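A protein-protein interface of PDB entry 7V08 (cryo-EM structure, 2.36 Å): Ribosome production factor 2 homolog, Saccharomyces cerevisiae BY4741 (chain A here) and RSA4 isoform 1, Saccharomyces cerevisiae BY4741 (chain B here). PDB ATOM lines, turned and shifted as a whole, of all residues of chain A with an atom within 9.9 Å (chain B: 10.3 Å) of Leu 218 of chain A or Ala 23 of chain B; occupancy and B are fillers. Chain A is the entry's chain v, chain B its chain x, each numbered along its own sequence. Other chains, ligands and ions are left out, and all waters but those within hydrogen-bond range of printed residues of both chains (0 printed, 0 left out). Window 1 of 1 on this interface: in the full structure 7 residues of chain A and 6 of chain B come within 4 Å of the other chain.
Of the 14 printed residues of chain A, 3 touch a printed residue of chain B. Printed residues of chain A that touch a printed residue of chain B: Lys 216, Arg 217 and Leu 218. Hydrophobic or aromatic side chains of chain B that line the printed part of chain A: Val 22 and Ile 24. Along chain B the printed residues that touch a printed residue of chain A span positions 22 to 99.
OD2 of Asp 99 of chain B is in salt-bridge range of NH1 of Arg 217 of chain A, 2.9 Å away.
No residue of chain B comes within 4 Å of Gly 214 of chain A. Of the printed residues of chain B, Lys 216 of chain A touches Asp 99 (3.2 Å). Of the printed residues of chain B, Arg 217 of chain A touches Asp 99 (2.9 Å). Leu 218 of chain A touches just these residues of chain B: Val 22 (3.8 Å), Ala 23 (3.7 Å) and Ile 24 (3.9 Å). No residue of chain B comes within 4 Å of Pro 219 of chain A. Printed residues of chain A within 4 Å of Ile 24 of chain B: Leu 218 (3.9 Å). Of the printed residues of chain A, Asp 99 of chain B touches Lys 216 (3.2 Å) and Arg 217 (2.9 Å). The nearest printed residue of chain A that does not touch Asp 99 of chain B is Gly 215 of chain A (6.5 Å).
The backbone carbonyl oxygen of Leu 218 of chain A lies within hydrogen-bond range of the side-chain hydroxyl of Ser 211 of chain A, at 3.3 Å.
CD of Lys 216 of chain A touches OD1 of Asp 99 of chain B, 3.2 Å away. CG1 of Val 22 of chain B touches CD1 of Leu 218 of chain A, at 3.8 Å. Ala 23 of chain B touches Leu 218 of chain A. CD1 of Leu 218 of chain A touches CD1 of Ile 24 of chain B, at 3.9 Å.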
ATOM      1  N   SER A 208      -8.414  18.753  -1.664  1.00  0.00           N
ATOM      2  CA  SER A 208      -9.663  18.158  -2.118  1.00  0.00           C
ATOM      3  C   SER A 208      -9.544  16.641  -2.144  1.00  0.00           C
ATOM      4  O   SER A 208      -8.478  16.096  -2.445  1.00  0.00           O
ATOM      5  CB  SER A 208     -10.057  18.688  -3.501  1.00  0.00           C
ATOM      6  OG  SER A 208      -9.021  18.498  -4.445  1.00  0.00           O
ATOM      7  N   TYR A 209     -10.646  15.968  -1.820  1.00  0.00           N
ATOM      8  CA  TYR A 209     -10.699  14.517  -1.786  1.00  0.00           C
ATOM      9  C   TYR A 209     -12.019  14.046  -2.375  1.00  0.00           C
ATOM     10  O   TYR A 209     -13.004  14.787  -2.416  1.00  0.00           O
ATOM     11  CB  TYR A 209     -10.549  13.974  -0.356  1.00  0.00           C
ATOM     12  CG  TYR A 209      -9.272  14.397   0.318  1.00  0.00           C
ATOM     13  CD1 TYR A 209      -8.100  13.673   0.146  1.00  0.00           C
ATOM     14  CD2 TYR A 209      -9.234  15.527   1.125  1.00  0.00           C
ATOM     15  CE1 TYR A 209      -6.929  14.061   0.760  1.00  0.00           C
ATOM     16  CE2 TYR A 209      -8.072  15.920   1.740  1.00  0.00           C
ATOM     17  CZ  TYR A 209      -6.921  15.184   1.555  1.00  0.00           C
ATOM     18  OH  TYR A 209      -5.759  15.580   2.173  1.00  0.00           O
ATOM     19  N   LYS A 210     -12.027  12.799  -2.835  1.00  0.00           N
ATOM     20  CA  LYS A 210     -13.269  12.166  -3.251  1.00  0.00           C
ATOM     21  C   LYS A 210     -14.164  11.949  -2.036  1.00  0.00           C
ATOM     22  O   LYS A 210     -13.724  11.430  -1.007  1.00  0.00           O
ATOM     23  CB  LYS A 210     -12.975  10.838  -3.945  1.00  0.00           C
ATOM     24  CG  LYS A 210     -14.201  10.102  -4.469  1.00  0.00           C
ATOM     25  CD  LYS A 210     -14.652  10.648  -5.814  1.00  0.00           C
ATOM     26  CE  LYS A 210     -15.951  10.002  -6.259  1.00  0.00           C
ATOM     27  NZ  LYS A 210     -15.806   8.558  -6.607  1.00  0.00           N
ATOM     28  N   SER A 211     -15.430  12.354  -2.154  1.00  0.00           N
ATOM     29  CA  SER A 211     -16.340  12.316  -1.019  1.00  0.00           C
ATOM     30  C   SER A 211     -17.180  11.050  -0.949  1.00  0.00           C
ATOM     31  O   SER A 211     -17.658  10.713   0.137  1.00  0.00           O
ATOM     32  CB  SER A 211     -17.284  13.525  -1.045  1.00  0.00           C
ATOM     33  OG  SER A 211     -18.362  13.310  -1.939  1.00  0.00           O
ATOM     34  N   ASP A 212     -17.401  10.369  -2.075  1.00  0.00           N
ATOM     35  CA  ASP A 212     -18.209   9.155  -2.196  1.00  0.00           C
ATOM     36  C   ASP A 212     -19.663   9.361  -1.777  1.00  0.00           C
ATOM     37  O   ASP A 212     -20.440   8.400  -1.752  1.00  0.00           O
ATOM     38  CB  ASP A 212     -17.597   7.987  -1.405  1.00  0.00           C
ATOM     39  CG  ASP A 212     -17.921   6.630  -2.012  1.00  0.00           C
ATOM     40  OD1 ASP A 212     -18.519   6.592  -3.105  1.00  0.00           O
ATOM     41  OD2 ASP A 212     -17.571   5.601  -1.396  1.00  0.00           O
ATOM     42  N   GLN A 213     -20.054  10.592  -1.455  1.00  0.00           N
ATOM     43  CA  GLN A 213     -21.431  10.927  -1.122  1.00  0.00           C
ATOM     44  C   GLN A 213     -21.992  12.067  -1.947  1.00  0.00           C
ATOM     45  O   GLN A 213     -23.219  12.169  -2.061  1.00  0.00           O
ATOM     46  CB  GLN A 213     -21.557  11.299   0.361  1.00  0.00           C
ATOM     47  CG  GLN A 213     -21.435  10.134   1.323  1.00  0.00           C
ATOM     48  CD  GLN A 213     -21.482  10.583   2.770  1.00  0.00           C
ATOM     49  OE1 GLN A 213     -21.609  11.773   3.058  1.00  0.00           O
ATOM     50  NE2 GLN A 213     -21.382   9.631   3.690  1.00  0.00           N
ATOM     51  N   GLY A 214     -21.150  12.940  -2.494  1.00  0.00           N
ATOM     52  CA  GLY A 214     -21.598  13.997  -3.373  1.00  0.00           C
ATOM     53  C   GLY A 214     -21.266  13.716  -4.824  1.00  0.00           C
ATOM     54  O   GLY A 214     -21.301  14.621  -5.662  1.00  0.00           O
ATOM     55  N   GLY A 215     -20.936  12.464  -5.127  1.00  0.00           N
ATOM     56  CA  GLY A 215     -20.584  12.083  -6.476  1.00  0.00           C
ATOM     57  C   GLY A 215     -19.182  12.529  -6.845  1.00  0.00           C
ATOM     58  O   GLY A 215     -18.402  13.008  -6.018  1.00  0.00           O
ATOM     59  N   LYS A 216     -18.867  12.374  -8.127  1.00  0.00           N
ATOM     60  CA  LYS A 216     -17.576  12.781  -8.655  1.00  0.00           C
ATOM     61  C   LYS A 216     -17.521  14.266  -8.980  1.00  0.00           C
ATOM     62  O   LYS A 216     -16.440  14.784  -9.273  1.00  0.00           O
ATOM     63  CB  LYS A 216     -17.228  11.954  -9.896  1.00  0.00           C
ATOM     64  CG  LYS A 216     -18.237  12.052 -11.025  1.00  0.00           C
ATOM     65  CD  LYS A 216     -17.835  11.192 -12.223  1.00  0.00           C
ATOM     66  CE  LYS A 216     -16.448  11.554 -12.737  1.00  0.00           C
ATOM     67  NZ  LYS A 216     -16.318  13.011 -13.018  1.00  0.00           N
ATOM     68  N   ARG A 217     -18.655  14.962  -8.912  1.00  0.00           N
ATOM     69  CA  ARG A 217     -18.713  16.380  -9.229  1.00  0.00           C
ATOM     70  C   ARG A 217     -18.582  17.284  -8.012  1.00  0.00           C
ATOM     71  O   ARG A 217     -18.318  18.477  -8.182  1.00  0.00           O
ATOM     72  CB  ARG A 217     -20.026  16.711  -9.953  1.00  0.00           C
ATOM     73  CG  ARG A 217     -20.578  15.586 -10.829  1.00  0.00           C
ATOM     74  CD  ARG A 217     -19.660  15.242 -12.001  1.00  0.00           C
ATOM     75  NE  ARG A 217     -19.439  16.373 -12.889  1.00  0.00           N
ATOM     76  CZ  ARG A 217     -20.201  16.666 -13.933  1.00  0.00           C
ATOM     77  NH1 ARG A 217     -21.266  15.944 -14.234  1.00  0.00           N
ATOM     78  NH2 ARG A 217     -19.889  17.714 -14.689  1.00  0.00           N
ATOM     79  N   LEU A 218     -18.764  16.757  -6.803  1.00  0.00           N
ATOM     80  CA  LEU A 218     -18.665  17.539  -5.570  1.00  0.00           C
ATOM     81  C   LEU A 218     -17.684  16.866  -4.621  1.00  0.00           C
ATOM     82  O   LEU A 218     -17.984  15.791  -4.074  1.00  0.00           O
ATOM     83  CB  LEU A 218     -20.027  17.698  -4.912  1.00  0.00           C
ATOM     84  CG  LEU A 218     -21.103  18.344  -5.777  1.00  0.00           C
ATOM     85  CD1 LEU A 218     -22.467  18.165  -5.140  1.00  0.00           C
ATOM     86  CD2 LEU A 218     -20.791  19.810  -5.970  1.00  0.00           C
ATOM     87  N   PRO A 219     -16.507  17.449  -4.410  1.00  0.00           N
ATOM     88  CA  PRO A 219     -15.516  16.847  -3.520  1.00  0.00           C
ATOM     89  C   PRO A 219     -15.620  17.373  -2.095  1.00  0.00           C
ATOM     90  O   PRO A 219     -16.264  18.385  -1.816  1.00  0.00           O
ATOM     91  CB  PRO A 219     -14.192  17.285  -4.158  1.00  0.00           C
ATOM     92  CG  PRO A 219     -14.507  18.645  -4.675  1.00  0.00           C
ATOM     93  CD  PRO A 219     -15.967  18.637  -5.090  1.00  0.00           C
ATOM     94  N   ARG A 220     -14.956  16.660  -1.188  1.00  0.00           N
ATOM     95  CA  ARG A 220     -14.800  17.139   0.179  1.00  0.00           C
ATOM     96  C   ARG A 220     -13.584  18.051   0.276  1.00  0.00           C
ATOM     97  O   ARG A 220     -12.482  17.680  -0.138  1.00  0.00           O
ATOM     98  CB  ARG A 220     -14.652  15.967   1.146  1.00  0.00           C
ATOM     99  CG  ARG A 220     -14.307  16.363   2.581  1.00  0.00           C
ATOM    100  CD  ARG A 220     -15.528  16.840   3.354  1.00  0.00           C
ATOM    101  NE  ARG A 220     -15.235  17.007   4.773  1.00  0.00           N
ATOM    102  CZ  ARG A 220     -16.111  17.406   5.685  1.00  0.00           C
ATOM    103  NH1 ARG A 220     -17.358  17.709   5.362  1.00  0.00           N
ATOM    104  NH2 ARG A 220     -15.728  17.501   6.954  1.00  0.00           N
ATOM    105  N   ILE A 221     -13.782  19.238   0.831  1.00  0.00           N
ATOM    106  CA  ILE A 221     -12.728  20.234   0.978  1.00  0.00           C
ATOM    107  C   ILE A 221     -12.163  20.140   2.386  1.00  0.00           C
ATOM    108  O   ILE A 221     -12.889  19.839   3.337  1.00  0.00           O
ATOM    109  CB  ILE A 221     -13.268  21.647   0.679  1.00  0.00           C
ATOM    110  CG1 ILE A 221     -13.907  21.668  -0.706  1.00  0.00           C
ATOM    111  CG2 ILE A 221     -12.162  22.689   0.734  1.00  0.00           C
ATOM    112  CD1 ILE A 221     -12.961  21.246  -1.796  1.00  0.00           C
ATOM    113  N   ARG B  20     -26.553  30.089  -6.805  1.00  0.00           N
ATOM    114  CA  ARG B  20     -26.702  28.881  -7.600  1.00  0.00           C
ATOM    115  C   ARG B  20     -27.228  27.743  -6.741  1.00  0.00           C
ATOM    116  O   ARG B  20     -27.014  27.707  -5.527  1.00  0.00           O
ATOM    117  CB  ARG B  20     -25.368  28.466  -8.229  1.00  0.00           C
ATOM    118  CG  ARG B  20     -24.577  29.599  -8.871  1.00  0.00           C
ATOM    119  CD  ARG B  20     -25.134  29.952 -10.234  1.00  0.00           C
ATOM    120  NE  ARG B  20     -25.416  28.758 -11.020  1.00  0.00           N
ATOM    121  CZ  ARG B  20     -25.849  28.772 -12.273  1.00  0.00           C
ATOM    122  NH1 ARG B  20     -26.045  29.906 -12.923  1.00  0.00           N
ATOM    123  NH2 ARG B  20     -26.087  27.616 -12.890  1.00  0.00           N
ATOM    124  N   GLU B  21     -27.927  26.813  -7.384  1.00  0.00           N
ATOM    125  CA  GLU B  21     -28.383  25.615  -6.699  1.00  0.00           C
ATOM    126  C   GLU B  21     -27.409  24.467  -6.935  1.00  0.00           C
ATOM    127  O   GLU B  21     -26.807  24.340  -8.006  1.00  0.00           O
ATOM    128  CB  GLU B  21     -29.790  25.231  -7.162  1.00  0.00           C
ATOM    129  CG  GLU B  21     -29.899  24.869  -8.633  1.00  0.00           C
ATOM    130  CD  GLU B  21     -31.328  24.612  -9.078  1.00  0.00           C
ATOM    131  OE1 GLU B  21     -32.199  24.378  -8.216  1.00  0.00           O
ATOM    132  OE2 GLU B  21     -31.585  24.656 -10.300  1.00  0.00           O
ATOM    133  N   VAL B  22     -27.265  23.617  -5.922  1.00  0.00           N
ATOM    134  CA  VAL B  22     -26.313  22.514  -5.943  1.00  0.00           C
ATOM    135  C   VAL B  22     -27.075  21.229  -6.224  1.00  0.00           C
ATOM    136  O   VAL B  22     -28.029  20.898  -5.512  1.00  0.00           O
ATOM    137  CB  VAL B  22     -25.529  22.416  -4.621  1.00  0.00           C
ATOM    138  CG1 VAL B  22     -24.692  21.143  -4.576  1.00  0.00           C
ATOM    139  CG2 VAL B  22     -24.639  23.630  -4.456  1.00  0.00           C
ATOM    140  N   ALA B  23     -26.656  20.513  -7.265  1.00  0.00           N
ATOM    141  CA  ALA B  23     -27.274  19.244  -7.644  1.00  0.00           C
ATOM    142  C   ALA B  23     -26.777  18.174  -6.681  1.00  0.00           C
ATOM    143  O   ALA B  23     -25.712  17.584  -6.865  1.00  0.00           O
ATOM    144  CB  ALA B  23     -26.950  18.896  -9.091  1.00  0.00           C
ATOM    145  N   ILE B  24     -27.565  17.925  -5.639  1.00  0.00           N
ATOM    146  CA  ILE B  24     -27.172  17.042  -4.550  1.00  0.00           C
ATOM    147  C   ILE B  24     -27.983  15.757  -4.638  1.00  0.00           C
ATOM    148  O   ILE B  24     -29.081  15.722  -5.206  1.00  0.00           O
ATOM    149  CB  ILE B  24     -27.348  17.728  -3.175  1.00  0.00           C
ATOM    150  CG1 ILE B  24     -26.488  17.051  -2.107  1.00  0.00           C
ATOM    151  CG2 ILE B  24     -28.805  17.734  -2.751  1.00  0.00           C
ATOM    152  CD1 ILE B  24     -25.005  17.271  -2.284  1.00  0.00           C
ATOM    153  N   ILE B  25     -27.418  14.689  -4.098  1.00  0.00           N
ATOM    154  CA  ILE B  25     -28.099  13.396  -4.074  1.00  0.00           C
ATOM    155  C   ILE B  25     -28.823  13.243  -2.738  1.00  0.00           C
ATOM    156  O   ILE B  25     -28.175  13.308  -1.682  1.00  0.00           O
ATOM    157  CB  ILE B  25     -27.101  12.266  -4.294  1.00  0.00           C
ATOM    158  CG1 ILE B  25     -26.046  12.700  -5.319  1.00  0.00           C
ATOM    159  CG2 ILE B  25     -27.821  11.024  -4.777  1.00  0.00           C
ATOM    160  CD1 ILE B  25     -25.151  11.574  -5.806  1.00  0.00           C
ATOM    161  N   PRO B  26     -30.141  13.057  -2.739  1.00  0.00           N
ATOM    162  CA  PRO B  26     -30.858  12.845  -1.476  1.00  0.00           C
ATOM    163  C   PRO B  26     -30.430  11.549  -0.804  1.00  0.00           C
ATOM    164  O   PRO B  26     -30.065  10.569  -1.460  1.00  0.00           O
ATOM    165  CB  PRO B  26     -32.329  12.786  -1.904  1.00  0.00           C
ATOM    166  CG  PRO B  26     -32.366  13.422  -3.268  1.00  0.00           C
ATOM    167  CD  PRO B  26     -31.052  13.100  -3.894  1.00  0.00           C
ATOM    168  N   ASP B  99     -22.961   9.570 -14.458  1.00  0.00           N
ATOM    169  CA  ASP B  99     -22.365   9.621 -13.130  1.00  0.00           C
ATOM    170  C   ASP B  99     -23.090   8.730 -12.140  1.00  0.00           C
ATOM    171  O   ASP B  99     -22.451   7.934 -11.443  1.00  0.00           O
ATOM    172  CB  ASP B  99     -22.347  11.071 -12.617  1.00  0.00           C
ATOM    173  CG  ASP B  99     -21.449  11.972 -13.444  1.00  0.00           C
ATOM    174  OD1 ASP B  99     -20.478  11.465 -14.036  1.00  0.00           O
ATOM    175  OD2 ASP B  99     -21.715  13.188 -13.508  1.00  0.00           O
ATOM    176  N   ASN B 100     -24.410   8.848 -12.057  1.00  0.00           N
ATOM    177  CA  ASN B 100     -25.217   7.974 -11.225  1.00  0.00           C
ATOM    178  C   ASN B 100     -26.616   7.904 -11.814  1.00  0.00           C
ATOM    179  O   ASN B 100     -26.998   8.720 -12.657  1.00  0.00           O
ATOM    180  CB  ASN B 100     -25.253   8.450  -9.768  1.00  0.00           C
ATOM    181  CG  ASN B 100     -25.603   9.914  -9.638  1.00  0.00           C
ATOM    182  OD1 ASN B 100     -26.774  10.290  -9.678  1.00  0.00           O
ATOM    183  ND2 ASN B 100     -24.590  10.748  -9.457  1.00  0.00           N
ATOM    184  N   TYR B 102     -29.495   8.424 -10.365  1.00  0.00           N
ATOM    185  CA  TYR B 102     -30.367   9.525  -9.965  1.00  0.00           C
ATOM    186  C   TYR B 102     -30.166  10.740 -10.861  1.00  0.00           C
ATOM    187  O   TYR B 102     -31.132  11.312 -11.374  1.00  0.00           O
ATOM    188  CB  TYR B 102     -30.127   9.887  -8.501  1.00  0.00           C
ATOM    189  CG  TYR B 102     -30.880  11.123  -8.050  1.00  0.00           C
ATOM    190  CD1 TYR B 102     -32.249  11.086  -7.837  1.00  0.00           C
ATOM    191  CD2 TYR B 102     -30.219  12.324  -7.845  1.00  0.00           C
ATOM    192  CE1 TYR B 102     -32.941  12.210  -7.419  1.00  0.00           C
ATOM    193  CE2 TYR B 102     -30.897  13.453  -7.432  1.00  0.00           C
ATOM    194  CZ  TYR B 102     -32.260  13.390  -7.224  1.00  0.00           C
ATOM    195  OH  TYR B 102     -32.940  14.508  -6.813  1.00  0.00           O
ATOM    196  N   SER B 103     -28.911  11.138 -11.075  1.00  0.00           N
ATOM    197  CA  SER B 103     -28.642  12.280 -11.942  1.00  0.00           C
ATOM    198  C   SER B 103     -28.965  11.974 -13.399  1.00  0.00           C
ATOM    199  O   SER B 103     -29.457  12.851 -14.120  1.00  0.00           O
ATOM    200  CB  SER B 103     -27.184  12.717 -11.805  1.00  0.00           C
ATOM    201  OG  SER B 103     -26.301  11.671 -12.167  1.00  0.00           O
ATOM    202  N   SER B 104     -28.716  10.741 -13.847  1.00  0.00           N
ATOM    203  CA  SER B 104     -28.934  10.411 -15.250  1.00  0.00           C
ATOM    204  C   SER B 104     -30.415  10.369 -15.596  1.00  0.00           C
ATOM    205  O   SER B 104     -30.834  10.935 -16.611  1.00  0.00           O
ATOM    206  CB  SER B 104     -28.274   9.074 -15.583  1.00  0.00           C
ATOM    207  OG  SER B 104     -26.870   9.137 -15.408  1.00  0.00           O
ATOM    208  N   LYS B 107     -33.259  12.509 -11.797  1.00  0.00           N
ATOM    209  CA  LYS B 107     -33.193  13.951 -11.561  1.00  0.00           C
ATOM    210  C   LYS B 107     -34.012  14.776 -12.557  1.00  0.00           C
ATOM    211  O   LYS B 107     -34.721  15.692 -12.105  1.00  0.00           O
ATOM    212  CB  LYS B 107     -31.726  14.406 -11.521  1.00  0.00           C
ATOM    213  CG  LYS B 107     -31.528  15.896 -11.337  1.00  0.00           C
ATOM    214  CD  LYS B 107     -30.078  16.285 -11.580  1.00  0.00           C
ATOM    215  CE  LYS B 107     -29.878  17.786 -11.444  1.00  0.00           C
ATOM    216  NZ  LYS B 107     -28.549  18.215 -11.974  1.00  0.00           N
ATOM    217  N   PRO B 108     -33.985  14.529 -13.875  1.00  0.00           N
ATOM    218  CA  PRO B 108     -34.971  15.193 -14.746  1.00  0.00           C
ATOM    219  C   PRO B 108     -36.402  14.728 -14.512  1.00  0.00           C
ATOM    220  O   PRO B 108     -37.337  15.429 -14.919  1.00  0.00           O
ATOM    221  CB  PRO B 108     -34.490  14.843 -16.162  1.00  0.00           C
ATOM    222  CG  PRO B 108     -33.045  14.524 -16.001  1.00  0.00           C
ATOM    223  CD  PRO B 108     -32.974  13.819 -14.684  1.00  0.00           C
